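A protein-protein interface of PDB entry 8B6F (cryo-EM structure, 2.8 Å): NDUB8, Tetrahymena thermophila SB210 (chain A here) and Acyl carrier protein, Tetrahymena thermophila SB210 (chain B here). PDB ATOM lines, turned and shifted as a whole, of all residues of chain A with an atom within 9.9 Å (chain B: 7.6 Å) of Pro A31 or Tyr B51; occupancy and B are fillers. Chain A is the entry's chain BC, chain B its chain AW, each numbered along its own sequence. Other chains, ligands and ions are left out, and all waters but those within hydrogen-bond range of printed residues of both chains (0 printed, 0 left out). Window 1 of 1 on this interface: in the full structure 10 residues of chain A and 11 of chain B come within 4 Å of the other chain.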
ATOM      1  N   GLY A  27       3.079  22.543 -10.805  1.00  0.00           N
ATOM      2  CA  GLY A  27       3.047  21.868 -12.135  1.00  0.00           C
ATOM      3  C   GLY A  27       1.708  22.004 -12.837  1.00  0.00           C
ATOM      4  O   GLY A  27       1.612  22.629 -13.892  1.00  0.00           O
ATOM      5  N   TRP A  28       0.674  21.409 -12.250  1.00  0.00           N
ATOM      6  CA  TRP A  28      -0.665  21.500 -12.810  1.00  0.00           C
ATOM      7  C   TRP A  28      -1.173  22.934 -12.700  1.00  0.00           C
ATOM      8  O   TRP A  28      -0.848  23.649 -11.750  1.00  0.00           O
ATOM      9  CB  TRP A  28      -1.586  20.530 -12.066  1.00  0.00           C
ATOM     10  CG  TRP A  28      -3.000  20.515 -12.519  1.00  0.00           C
ATOM     11  CD1 TRP A  28      -4.026  21.259 -12.025  1.00  0.00           C
ATOM     12  CD2 TRP A  28      -3.552  19.706 -13.560  1.00  0.00           C
ATOM     13  NE1 TRP A  28      -5.188  20.966 -12.696  1.00  0.00           N
ATOM     14  CE2 TRP A  28      -4.922  20.014 -13.645  1.00  0.00           C
ATOM     15  CE3 TRP A  28      -3.019  18.754 -14.432  1.00  0.00           C
ATOM     16  CZ2 TRP A  28      -5.767  19.404 -14.565  1.00  0.00           C
ATOM     17  CZ3 TRP A  28      -3.859  18.145 -15.342  1.00  0.00           C
ATOM     18  CH2 TRP A  28      -5.220  18.474 -15.403  1.00  0.00           C
ATOM     19  N   ASP A  29      -1.976  23.365 -13.676  1.00  0.00           N
ATOM     20  CA  ASP A  29      -2.556  24.704 -13.589  1.00  0.00           C
ATOM     21  C   ASP A  29      -3.864  24.587 -12.822  1.00  0.00           C
ATOM     22  O   ASP A  29      -4.882  24.153 -13.365  1.00  0.00           O
ATOM     23  CB  ASP A  29      -2.791  25.261 -14.990  1.00  0.00           C
ATOM     24  CG  ASP A  29      -2.756  26.771 -15.038  1.00  0.00           C
ATOM     25  OD1 ASP A  29      -2.558  27.404 -13.980  1.00  0.00           O
ATOM     26  OD2 ASP A  29      -2.936  27.327 -16.141  1.00  0.00           O
ATOM     27  N   ARG A  30      -3.831  24.974 -11.557  1.00  0.00           N
ATOM     28  CA  ARG A  30      -4.996  24.780 -10.716  1.00  0.00           C
ATOM     29  C   ARG A  30      -6.122  25.757 -11.060  1.00  0.00           C
ATOM     30  O   ARG A  30      -5.859  26.918 -11.387  1.00  0.00           O
ATOM     31  CB  ARG A  30      -4.581  24.925  -9.256  1.00  0.00           C
ATOM     32  CG  ARG A  30      -3.653  23.800  -8.820  1.00  0.00           C
ATOM     33  CD  ARG A  30      -3.003  24.066  -7.479  1.00  0.00           C
ATOM     34  NE  ARG A  30      -3.971  24.476  -6.472  1.00  0.00           N
ATOM     35  CZ  ARG A  30      -4.800  23.647  -5.853  1.00  0.00           C
ATOM     36  NH1 ARG A  30      -4.803  22.351  -6.114  1.00  0.00           N
ATOM     37  NH2 ARG A  30      -5.643  24.131  -4.949  1.00  0.00           N
ATOM     38  N   PRO A  31      -7.376  25.325 -10.992  1.00  0.00           N
ATOM     39  CA  PRO A  31      -8.499  26.247 -11.198  1.00  0.00           C
ATOM     40  C   PRO A  31      -8.587  27.229 -10.032  1.00  0.00           C
ATOM     41  O   PRO A  31      -8.085  26.968  -8.937  1.00  0.00           O
ATOM     42  CB  PRO A  31      -9.724  25.329 -11.306  1.00  0.00           C
ATOM     43  CG  PRO A  31      -9.335  24.085 -10.662  1.00  0.00           C
ATOM     44  CD  PRO A  31      -7.845  23.941 -10.844  1.00  0.00           C
ATOM     45  N   ASP A  32      -9.229  28.373 -10.265  1.00  0.00           N
ATOM     46  CA  ASP A  32      -9.244  29.434  -9.262  1.00  0.00           C
ATOM     47  C   ASP A  32      -9.949  28.939  -8.003  1.00  0.00           C
ATOM     48  O   ASP A  32     -10.823  28.070  -8.065  1.00  0.00           O
ATOM     49  CB  ASP A  32      -9.959  30.679  -9.789  1.00  0.00           C
ATOM     50  CG  ASP A  32      -8.999  31.732 -10.300  1.00  0.00           C
ATOM     51  OD1 ASP A  32      -7.870  31.371 -10.692  1.00  0.00           O
ATOM     52  OD2 ASP A  32      -9.373  32.924 -10.307  1.00  0.00           O
ATOM     53  N   VAL A  33      -9.561  29.483  -6.850  1.00  0.00           N
ATOM     54  CA  VAL A  33      -9.959  28.888  -5.574  1.00  0.00           C
ATOM     55  C   VAL A  33     -11.473  28.724  -5.551  1.00  0.00           C
ATOM     56  O   VAL A  33     -12.213  29.641  -5.931  1.00  0.00           O
ATOM     57  CB  VAL A  33      -9.499  29.768  -4.396  1.00  0.00           C
ATOM     58  CG1 VAL A  33     -10.143  29.338  -3.076  1.00  0.00           C
ATOM     59  CG2 VAL A  33      -7.985  29.768  -4.273  1.00  0.00           C
ATOM     60  N   PRO A  34     -11.967  27.567  -5.113  1.00  0.00           N
ATOM     61  CA  PRO A  34     -13.406  27.296  -5.184  1.00  0.00           C
ATOM     62  C   PRO A  34     -14.270  28.153  -4.275  1.00  0.00           C
ATOM     63  O   PRO A  34     -13.896  28.470  -3.144  1.00  0.00           O
ATOM     64  CB  PRO A  34     -13.497  25.821  -4.779  1.00  0.00           C
ATOM     65  CG  PRO A  34     -12.330  25.620  -3.900  1.00  0.00           C
ATOM     66  CD  PRO A  34     -11.238  26.430  -4.521  1.00  0.00           C
ATOM     67  N   LEU A  35     -15.441  28.526  -4.789  1.00  0.00           N
ATOM     68  CA  LEU A  35     -16.418  29.258  -3.994  1.00  0.00           C
ATOM     69  C   LEU A  35     -16.960  28.331  -2.911  1.00  0.00           C
ATOM     70  O   LEU A  35     -17.518  28.794  -1.911  1.00  0.00           O
ATOM     71  CB  LEU A  35     -17.518  29.844  -4.877  1.00  0.00           C
ATOM     72  CG  LEU A  35     -17.062  31.161  -5.516  1.00  0.00           C
ATOM     73  CD1 LEU A  35     -17.773  31.429  -6.826  1.00  0.00           C
ATOM     74  CD2 LEU A  35     -17.262  32.328  -4.556  1.00  0.00           C
ATOM     75  N   SER A  36     -16.787  27.022  -3.130  1.00  0.00           N
ATOM     76  CA  SER A  36     -17.173  25.944  -2.225  1.00  0.00           C
ATOM     77  C   SER A  36     -16.386  26.011  -0.927  1.00  0.00           C
ATOM     78  O   SER A  36     -16.813  25.430   0.077  1.00  0.00           O
ATOM     79  CB  SER A  36     -16.981  24.583  -2.896  1.00  0.00           C
ATOM     80  OG  SER A  36     -15.782  23.962  -2.468  1.00  0.00           O
ATOM     81  N   PHE A  37     -15.243  26.696  -0.932  1.00  0.00           N
ATOM     82  CA  PHE A  37     -14.419  26.786   0.266  1.00  0.00           C
ATOM     83  C   PHE A  37     -15.252  27.418   1.371  1.00  0.00           C
ATOM     84  O   PHE A  37     -15.184  26.992   2.529  1.00  0.00           O
ATOM     85  CB  PHE A  37     -13.157  27.592  -0.064  1.00  0.00           C
ATOM     86  CG  PHE A  37     -12.271  27.905   1.113  1.00  0.00           C
ATOM     87  CD1 PHE A  37     -12.579  28.938   1.984  1.00  0.00           C
ATOM     88  CD2 PHE A  37     -11.099  27.196   1.314  1.00  0.00           C
ATOM     89  CE1 PHE A  37     -11.749  29.237   3.049  1.00  0.00           C
ATOM     90  CE2 PHE A  37     -10.268  27.488   2.379  1.00  0.00           C
ATOM     91  CZ  PHE A  37     -10.593  28.511   3.246  1.00  0.00           C
ATOM     92  N   ARG B  44     -13.401  34.912 -12.107  1.00  0.00           N
ATOM     93  CA  ARG B  44     -12.849  33.618 -11.730  1.00  0.00           C
ATOM     94  C   ARG B  44     -12.653  32.750 -12.965  1.00  0.00           C
ATOM     95  O   ARG B  44     -13.537  32.658 -13.822  1.00  0.00           O
ATOM     96  CB  ARG B  44     -13.775  32.919 -10.736  1.00  0.00           C
ATOM     97  CG  ARG B  44     -13.912  33.647  -9.411  1.00  0.00           C
ATOM     98  CD  ARG B  44     -14.868  32.933  -8.466  1.00  0.00           C
ATOM     99  NE  ARG B  44     -14.432  31.577  -8.150  1.00  0.00           N
ATOM    100  CZ  ARG B  44     -14.803  30.489  -8.812  1.00  0.00           C
ATOM    101  NH1 ARG B  44     -15.624  30.554  -9.848  1.00  0.00           N
ATOM    102  NH2 ARG B  44     -14.338  29.305  -8.426  1.00  0.00           N
ATOM    103  N   ASN B  45     -11.494  32.109 -13.051  1.00  0.00           N
ATOM    104  CA  ASN B  45     -11.112  31.301 -14.207  1.00  0.00           C
ATOM    105  C   ASN B  45     -11.059  29.840 -13.772  1.00  0.00           C
ATOM    106  O   ASN B  45     -10.035  29.356 -13.289  1.00  0.00           O
ATOM    107  CB  ASN B  45      -9.775  31.764 -14.776  1.00  0.00           C
ATOM    108  CG  ASN B  45      -9.351  30.965 -15.992  1.00  0.00           C
ATOM    109  OD1 ASN B  45     -10.158  30.265 -16.599  1.00  0.00           O
ATOM    110  ND2 ASN B  45      -8.080  31.073 -16.355  1.00  0.00           N
ATOM    111  N   GLU B  46     -12.176  29.137 -13.953  1.00  0.00           N
ATOM    112  CA  GLU B  46     -12.249  27.700 -13.695  1.00  0.00           C
ATOM    113  C   GLU B  46     -11.666  26.983 -14.909  1.00  0.00           C
ATOM    114  O   GLU B  46     -12.374  26.533 -15.814  1.00  0.00           O
ATOM    115  CB  GLU B  46     -13.684  27.275 -13.415  1.00  0.00           C
ATOM    116  CG  GLU B  46     -14.310  27.997 -12.233  1.00  0.00           C
ATOM    117  CD  GLU B  46     -15.740  27.569 -11.982  1.00  0.00           C
ATOM    118  OE1 GLU B  46     -16.248  26.718 -12.740  1.00  0.00           O
ATOM    119  OE2 GLU B  46     -16.357  28.083 -11.026  1.00  0.00           O
ATOM    120  N   LYS B  47     -10.337  26.879 -14.919  1.00  0.00           N
ATOM    121  CA  LYS B  47      -9.637  26.314 -16.068  1.00  0.00           C
ATOM    122  C   LYS B  47     -10.157  24.918 -16.390  1.00  0.00           C
ATOM    123  O   LYS B  47     -10.734  24.680 -17.457  1.00  0.00           O
ATOM    124  CB  LYS B  47      -8.134  26.277 -15.787  1.00  0.00           C
ATOM    125  CG  LYS B  47      -7.535  27.624 -15.398  1.00  0.00           C
ATOM    126  CD  LYS B  47      -6.153  27.457 -14.788  1.00  0.00           C
ATOM    127  CE  LYS B  47      -5.589  28.787 -14.319  1.00  0.00           C
ATOM    128  NZ  LYS B  47      -5.287  29.698 -15.460  1.00  0.00           N
ATOM    129  N   SER B  48      -9.963  23.982 -15.468  1.00  0.00           N
ATOM    130  CA  SER B  48     -10.525  22.645 -15.563  1.00  0.00           C
ATOM    131  C   SER B  48     -10.904  22.205 -14.159  1.00  0.00           C
ATOM    132  O   SER B  48     -10.144  22.415 -13.212  1.00  0.00           O
ATOM    133  CB  SER B  48      -9.540  21.656 -16.197  1.00  0.00           C
ATOM    134  OG  SER B  48      -8.287  21.681 -15.537  1.00  0.00           O
ATOM    135  N   GLY B  49     -12.073  21.588 -14.031  1.00  0.00           N
ATOM    136  CA  GLY B  49     -12.602  21.228 -12.729  1.00  0.00           C
ATOM    137  C   GLY B  49     -11.616  20.514 -11.826  1.00  0.00           C
ATOM    138  O   GLY B  49     -11.778  20.518 -10.603  1.00  0.00           O
ATOM    139  N   TYR B  50     -10.593  19.900 -12.411  1.00  0.00           N
ATOM    140  CA  TYR B  50      -9.608  19.148 -11.646  1.00  0.00           C
ATOM    141  C   TYR B  50      -8.611  20.101 -10.999  1.00  0.00           C
ATOM    142  O   TYR B  50      -7.978  20.909 -11.686  1.00  0.00           O
ATOM    143  CB  TYR B  50      -8.880  18.161 -12.554  1.00  0.00           C
ATOM    144  CG  TYR B  50      -9.796  17.310 -13.397  1.00  0.00           C
ATOM    145  CD1 TYR B  50     -10.293  16.106 -12.921  1.00  0.00           C
ATOM    146  CD2 TYR B  50     -10.159  17.709 -14.676  1.00  0.00           C
ATOM    147  CE1 TYR B  50     -11.129  15.325 -13.692  1.00  0.00           C
ATOM    148  CE2 TYR B  50     -10.992  16.936 -15.454  1.00  0.00           C
ATOM    149  CZ  TYR B  50     -11.474  15.744 -14.958  1.00  0.00           C
ATOM    150  OH  TYR B  50     -12.307  14.970 -15.731  1.00  0.00           O
ATOM    151  N   TYR B  51      -8.472  20.006  -9.677  1.00  0.00           N
ATOM    152  CA  TYR B  51      -7.446  20.741  -8.950  1.00  0.00           C
ATOM    153  C   TYR B  51      -6.136  19.978  -8.848  1.00  0.00           C
ATOM    154  O   TYR B  51      -5.134  20.552  -8.409  1.00  0.00           O
ATOM    155  CB  TYR B  51      -7.943  21.095  -7.544  1.00  0.00           C
ATOM    156  CG  TYR B  51      -8.940  22.231  -7.513  1.00  0.00           C
ATOM    157  CD1 TYR B  51     -10.292  22.001  -7.718  1.00  0.00           C
ATOM    158  CD2 TYR B  51      -8.524  23.534  -7.271  1.00  0.00           C
ATOM    159  CE1 TYR B  51     -11.204  23.036  -7.690  1.00  0.00           C
ATOM    160  CE2 TYR B  51      -9.429  24.577  -7.238  1.00  0.00           C
ATOM    161  CZ  TYR B  51     -10.768  24.321  -7.447  1.00  0.00           C
ATOM    162  OH  TYR B  51     -11.675  25.355  -7.419  1.00  0.00           O
ATOM    163  N   ALA B  52      -6.117  18.709  -9.244  1.00  0.00           N
ATOM    164  CA  ALA B  52      -4.900  17.918  -9.290  1.00  0.00           C
ATOM    165  C   ALA B  52      -4.894  17.133 -10.590  1.00  0.00           C
ATOM    166  O   ALA B  52      -5.948  16.854 -11.165  1.00  0.00           O
ATOM    167  CB  ALA B  52      -4.789  16.966  -8.093  1.00  0.00           C
ATOM    168  N   ASN B  53      -3.700  16.780 -11.051  1.00  0.00           N
ATOM    169  CA  ASN B  53      -3.567  16.066 -12.313  1.00  0.00           C
ATOM    170  C   ASN B  53      -4.388  14.783 -12.253  1.00  0.00           C
ATOM    171  O   ASN B  53      -4.007  13.840 -11.550  1.00  0.00           O
ATOM    172  CB  ASN B  53      -2.098  15.760 -12.606  1.00  0.00           C
ATOM    173  CG  ASN B  53      -1.890  15.192 -13.992  1.00  0.00           C
ATOM    174  OD1 ASN B  53      -2.817  15.133 -14.797  1.00  0.00           O
ATOM    175  ND2 ASN B  53      -0.664  14.776 -14.283  1.00  0.00           N
ATOM    176  N   PRO B  54      -5.514  14.702 -12.968  1.00  0.00           N
ATOM    177  CA  PRO B  54      -6.354  13.498 -12.856  1.00  0.00           C
ATOM    178  C   PRO B  54      -5.642  12.231 -13.281  1.00  0.00           C
ATOM    179  O   PRO B  54      -5.908  11.164 -12.714  1.00  0.00           O
ATOM    180  CB  PRO B  54      -7.547  13.816 -13.768  1.00  0.00           C
ATOM    181  CG  PRO B  54      -7.044  14.829 -14.716  1.00  0.00           C
ATOM    182  CD  PRO B  54      -6.045  15.646 -13.966  1.00  0.00           C
ATOM    183  N   VAL B  57      -3.561  11.194 -10.355  1.00  0.00           N
ATOM    184  CA  VAL B  57      -4.451  10.727  -9.296  1.00  0.00           C
ATOM    185  C   VAL B  57      -4.931   9.314  -9.600  1.00  0.00           C
ATOM    186  O   VAL B  57      -4.929   8.436  -8.731  1.00  0.00           O
ATOM    187  CB  VAL B  57      -5.631  11.700  -9.118  1.00  0.00           C
ATOM    188  CG1 VAL B  57      -6.688  11.113  -8.190  1.00  0.00           C
ATOM    189  CG2 VAL B  57      -5.143  13.034  -8.583  1.00  0.00           C
ATOM    190  N   GLU B 124     -12.324  10.916 -10.132  1.00  0.00           N
ATOM    191  CA  GLU B 124     -12.928  12.207 -10.439  1.00  0.00           C
ATOM    192  C   GLU B 124     -13.138  13.021  -9.170  1.00  0.00           C
ATOM    193  O   GLU B 124     -12.797  14.207  -9.119  1.00  0.00           O
ATOM    194  CB  GLU B 124     -14.253  12.005 -11.175  1.00  0.00           C
ATOM    195  CG  GLU B 124     -14.092  11.605 -12.633  1.00  0.00           C
ATOM    196  CD  GLU B 124     -13.495  12.712 -13.481  1.00  0.00           C
ATOM    197  OE1 GLU B 124     -13.685  13.895 -13.132  1.00  0.00           O
ATOM    198  OE2 GLU B 124     -12.834  12.401 -14.494  1.00  0.00           O
ATOM    199  N   ILE B 126     -11.623  12.704  -6.232  1.00  0.00           N
ATOM    200  CA  ILE B 126     -10.347  13.050  -5.612  1.00  0.00           C
ATOM    201  C   ILE B 126      -9.675  14.185  -6.372  1.00  0.00           C
ATOM    202  O   ILE B 126      -9.161  15.135  -5.773  1.00  0.00           O
ATOM    203  CB  ILE B 126      -9.437  11.810  -5.526  1.00  0.00           C
ATOM    204  CG1 ILE B 126     -10.057  10.759  -4.603  1.00  0.00           C
ATOM    205  CG2 ILE B 126      -8.052  12.194  -5.021  1.00  0.00           C
ATOM    206  CD1 ILE B 126      -9.369   9.411  -4.655  1.00  0.00           C
ATOM    207  N   ALA B 127      -9.667  14.104  -7.705  1.00  0.00           N
ATOM    208  CA  ALA B 127      -9.004  15.131  -8.502  1.00  0.00           C
ATOM    209  C   ALA B 127      -9.716  16.472  -8.390  1.00  0.00           C
ATOM    210  O   ALA B 127      -9.065  17.518  -8.300  1.00  0.00           O
ATOM    211  CB  ALA B 127      -8.922  14.688  -9.961  1.00  0.00           C
ATOM    212  N   ARG B 128     -11.048  16.468  -8.404  1.00  0.00           N
ATOM    213  CA  ARG B 128     -11.800  17.710  -8.292  1.00  0.00           C
ATOM    214  C   ARG B 128     -11.842  18.251  -6.870  1.00  0.00           C
ATOM    215  O   ARG B 128     -12.256  19.398  -6.676  1.00  0.00           O
ATOM    216  CB  ARG B 128     -13.230  17.509  -8.798  1.00  0.00           C
ATOM    217  CG  ARG B 128     -13.313  17.119 -10.263  1.00  0.00           C
ATOM    218  CD  ARG B 128     -14.753  16.959 -10.713  1.00  0.00           C
ATOM    219  NE  ARG B 128     -14.839  16.432 -12.069  1.00  0.00           N
ATOM    220  CZ  ARG B 128     -14.770  17.169 -13.170  1.00  0.00           C
ATOM    221  NH1 ARG B 128     -14.608  18.480 -13.116  1.00  0.00           N
ATOM    222  NH2 ARG B 128     -14.866  16.574 -14.355  1.00  0.00           N
ATOM    223  N   ASN B 129     -11.434  17.462  -5.882  1.00  0.00           N
ATOM    224  CA  ASN B 129     -11.447  17.925  -4.503  1.00  0.00           C
ATOM    225  C   ASN B 129     -10.355  18.963  -4.279  1.00  0.00           C
ATOM    226  O   ASN B 129      -9.201  18.762  -4.666  1.00  0.00           O
ATOM    227  CB  ASN B 129     -11.262  16.744  -3.550  1.00  0.00           C
ATOM    228  CG  ASN B 129     -11.484  17.122  -2.097  1.00  0.00           C
ATOM    229  OD1 ASN B 129     -11.208  18.246  -1.684  1.00  0.00           O
ATOM    230  ND2 ASN B 129     -11.992  16.178  -1.316  1.00  0.00           N
ATOM    231  N   PHE B 130     -10.729  20.078  -3.658  1.00  0.00           N
ATOM    232  CA  PHE B 130      -9.771  21.070  -3.183  1.00  0.00           C
ATOM    233  C   PHE B 130      -9.194  20.555  -1.871  1.00  0.00           C
ATOM    234  O   PHE B 130      -9.914  20.445  -0.872  1.00  0.00           O
ATOM    235  CB  PHE B 130     -10.463  22.419  -3.006  1.00  0.00           C
ATOM    236  CG  PHE B 130      -9.523  23.574  -2.810  1.00  0.00           C
ATOM    237  CD1 PHE B 130      -8.954  24.212  -3.897  1.00  0.00           C
ATOM    238  CD2 PHE B 130      -9.237  24.046  -1.541  1.00  0.00           C
ATOM    239  CE1 PHE B 130      -8.105  25.288  -3.723  1.00  0.00           C
ATOM    240  CE2 PHE B 130      -8.387  25.121  -1.360  1.00  0.00           C
ATOM    241  CZ  PHE B 130      -7.819  25.741  -2.454  1.00  0.00           C
ATOM    242  N   PHE B 131      -7.900  20.230  -1.866  1.00  0.00           N
ATOM    243  CA  PHE B 131      -7.337  19.499  -0.735  1.00  0.00           C
ATOM    244  C   PHE B 131      -7.582  20.217   0.585  1.00  0.00           C
ATOM    245  O   PHE B 131      -7.691  19.566   1.629  1.00  0.00           O
ATOM    246  CB  PHE B 131      -5.840  19.265  -0.947  1.00  0.00           C
ATOM    247  CG  PHE B 131      -5.521  18.247  -2.016  1.00  0.00           C
ATOM    248  CD1 PHE B 131      -6.529  17.575  -2.696  1.00  0.00           C
ATOM    249  CD2 PHE B 131      -4.203  17.955  -2.329  1.00  0.00           C
ATOM    250  CE1 PHE B 131      -6.227  16.641  -3.669  1.00  0.00           C
ATOM    251  CE2 PHE B 131      -3.895  17.022  -3.300  1.00  0.00           C
ATOM    252  CZ  PHE B 131      -4.909  16.364  -3.972  1.00  0.00           C
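The backbone nitrogen (N) of Pro A34 sits close to the side-chain hydroxyl (OH) of Tyr B51 (3.2 Å).
N of Asp A32 is in hydrogen-bond range of O of Asn B45 (3.3 Å).
The guanidinium group (NH1) of Arg A30 lies within hydrogen-bond range of the backbone carbonyl oxygen (O) of Tyr B51 (2.9 Å).
The backbone carbonyl oxygen of Tyr B50 sits at hydrogen-bond distance from the indole nitrogen of Trp A28 (3.0 Å).
NZ of Lys B47 is in salt-bridge range of OD2 of Asp A29 (3.4 Å).
The side-chain hydroxyl (OH) of Tyr B51 is in hydrogen-bond range of the backbone carbonyl oxygen (O) of Asp A32 (2.9 Å).
The guanidinium group of Arg B44 lies within hydrogen-bond range of the backbone carbonyl oxygen of Val A33, 3.3 Å away.
Pro A31 touches just these residues of chain B: Lys B47 (3.98 Å), Ser B48 (3.2 Å), Tyr B50 (3.1 Å) and Tyr B51 (3.2 Å).
Of the printed residues of chain A, Phe B130 touches Arg A30 and Pro A34.
Of the printed residues of chain B, Leu A35 touches Arg B44.
Of the printed residues of chain A, Tyr B50 touches Trp A28 and Pro A31.
Phe A37 touches none of the printed residues of chain B.
Glu B46 touches none of the printed residues of chain A.
The nearest residue of chain B that does not touch Pro A31 is Asn B45 (4.05 Å).
The nearest printed residue of chain A that does not touch Asn B53 is Asp A29 (7.3 Å).
Tyr B51 touches Trp A28.
Arg A30 touches Lys B47.
Phe B130 touches Arg A30 (CE1 to NH2, 3.0 Å).
CG of Pro A31 touches O of Ser B48 (3.2 Å).
Tyr B51 touches Pro A31 (CE2 to O, 3.2 Å).
Arg B44 touches Asp A32.
Val A33 touches Tyr B51 (C to OH, 3.9 Å).
Pro A34 touches Arg B44.
Phe B130 touches Pro A34.
Arg B44 touches Leu A35.
Of the 11 printed residues of chain A, 8 touch a printed residue of chain B.
Hydrophobic or aromatic side chains of chain A within 4 Å of the printed part of chain B: Trp A28, Pro A31, Pro A34 and Leu A35.
Of the 19 printed residues of chain B, 9 touch a printed residue of chain A.
Printed residues of chain B that touch a printed residue of chain A: Arg B44, Asn B45, Lys B47, Ser B48, Tyr B50, Tyr B51, Asn B53, Pro B54 and Phe B130.
Hydrophobic or aromatic side chains of chain B that line the printed part of chain A: Tyr B50, Tyr B51, Pro B54 and Phe B130.
OH of Tyr B50 is in hydrogen-bond range of NH2 of Arg B128, 3.3 Å away.
The side-chain amino group (NZ) of Lys B47 sits close to the side-chain amide nitrogen (ND2) of Asn B45 (3.2 Å).
N of Tyr B51 lies within hydrogen-bond range of O of Ala B127 (2.9 Å).
The side-chain hydroxyl of Tyr B50 sits at hydrogen-bond distance from the side-chain carboxylate of Glu B124.
The guanidinium group (NH1) of Arg B44 lies within salt-bridge range of the side-chain carboxylate (OE2) of Glu B46 (2.8 Å).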
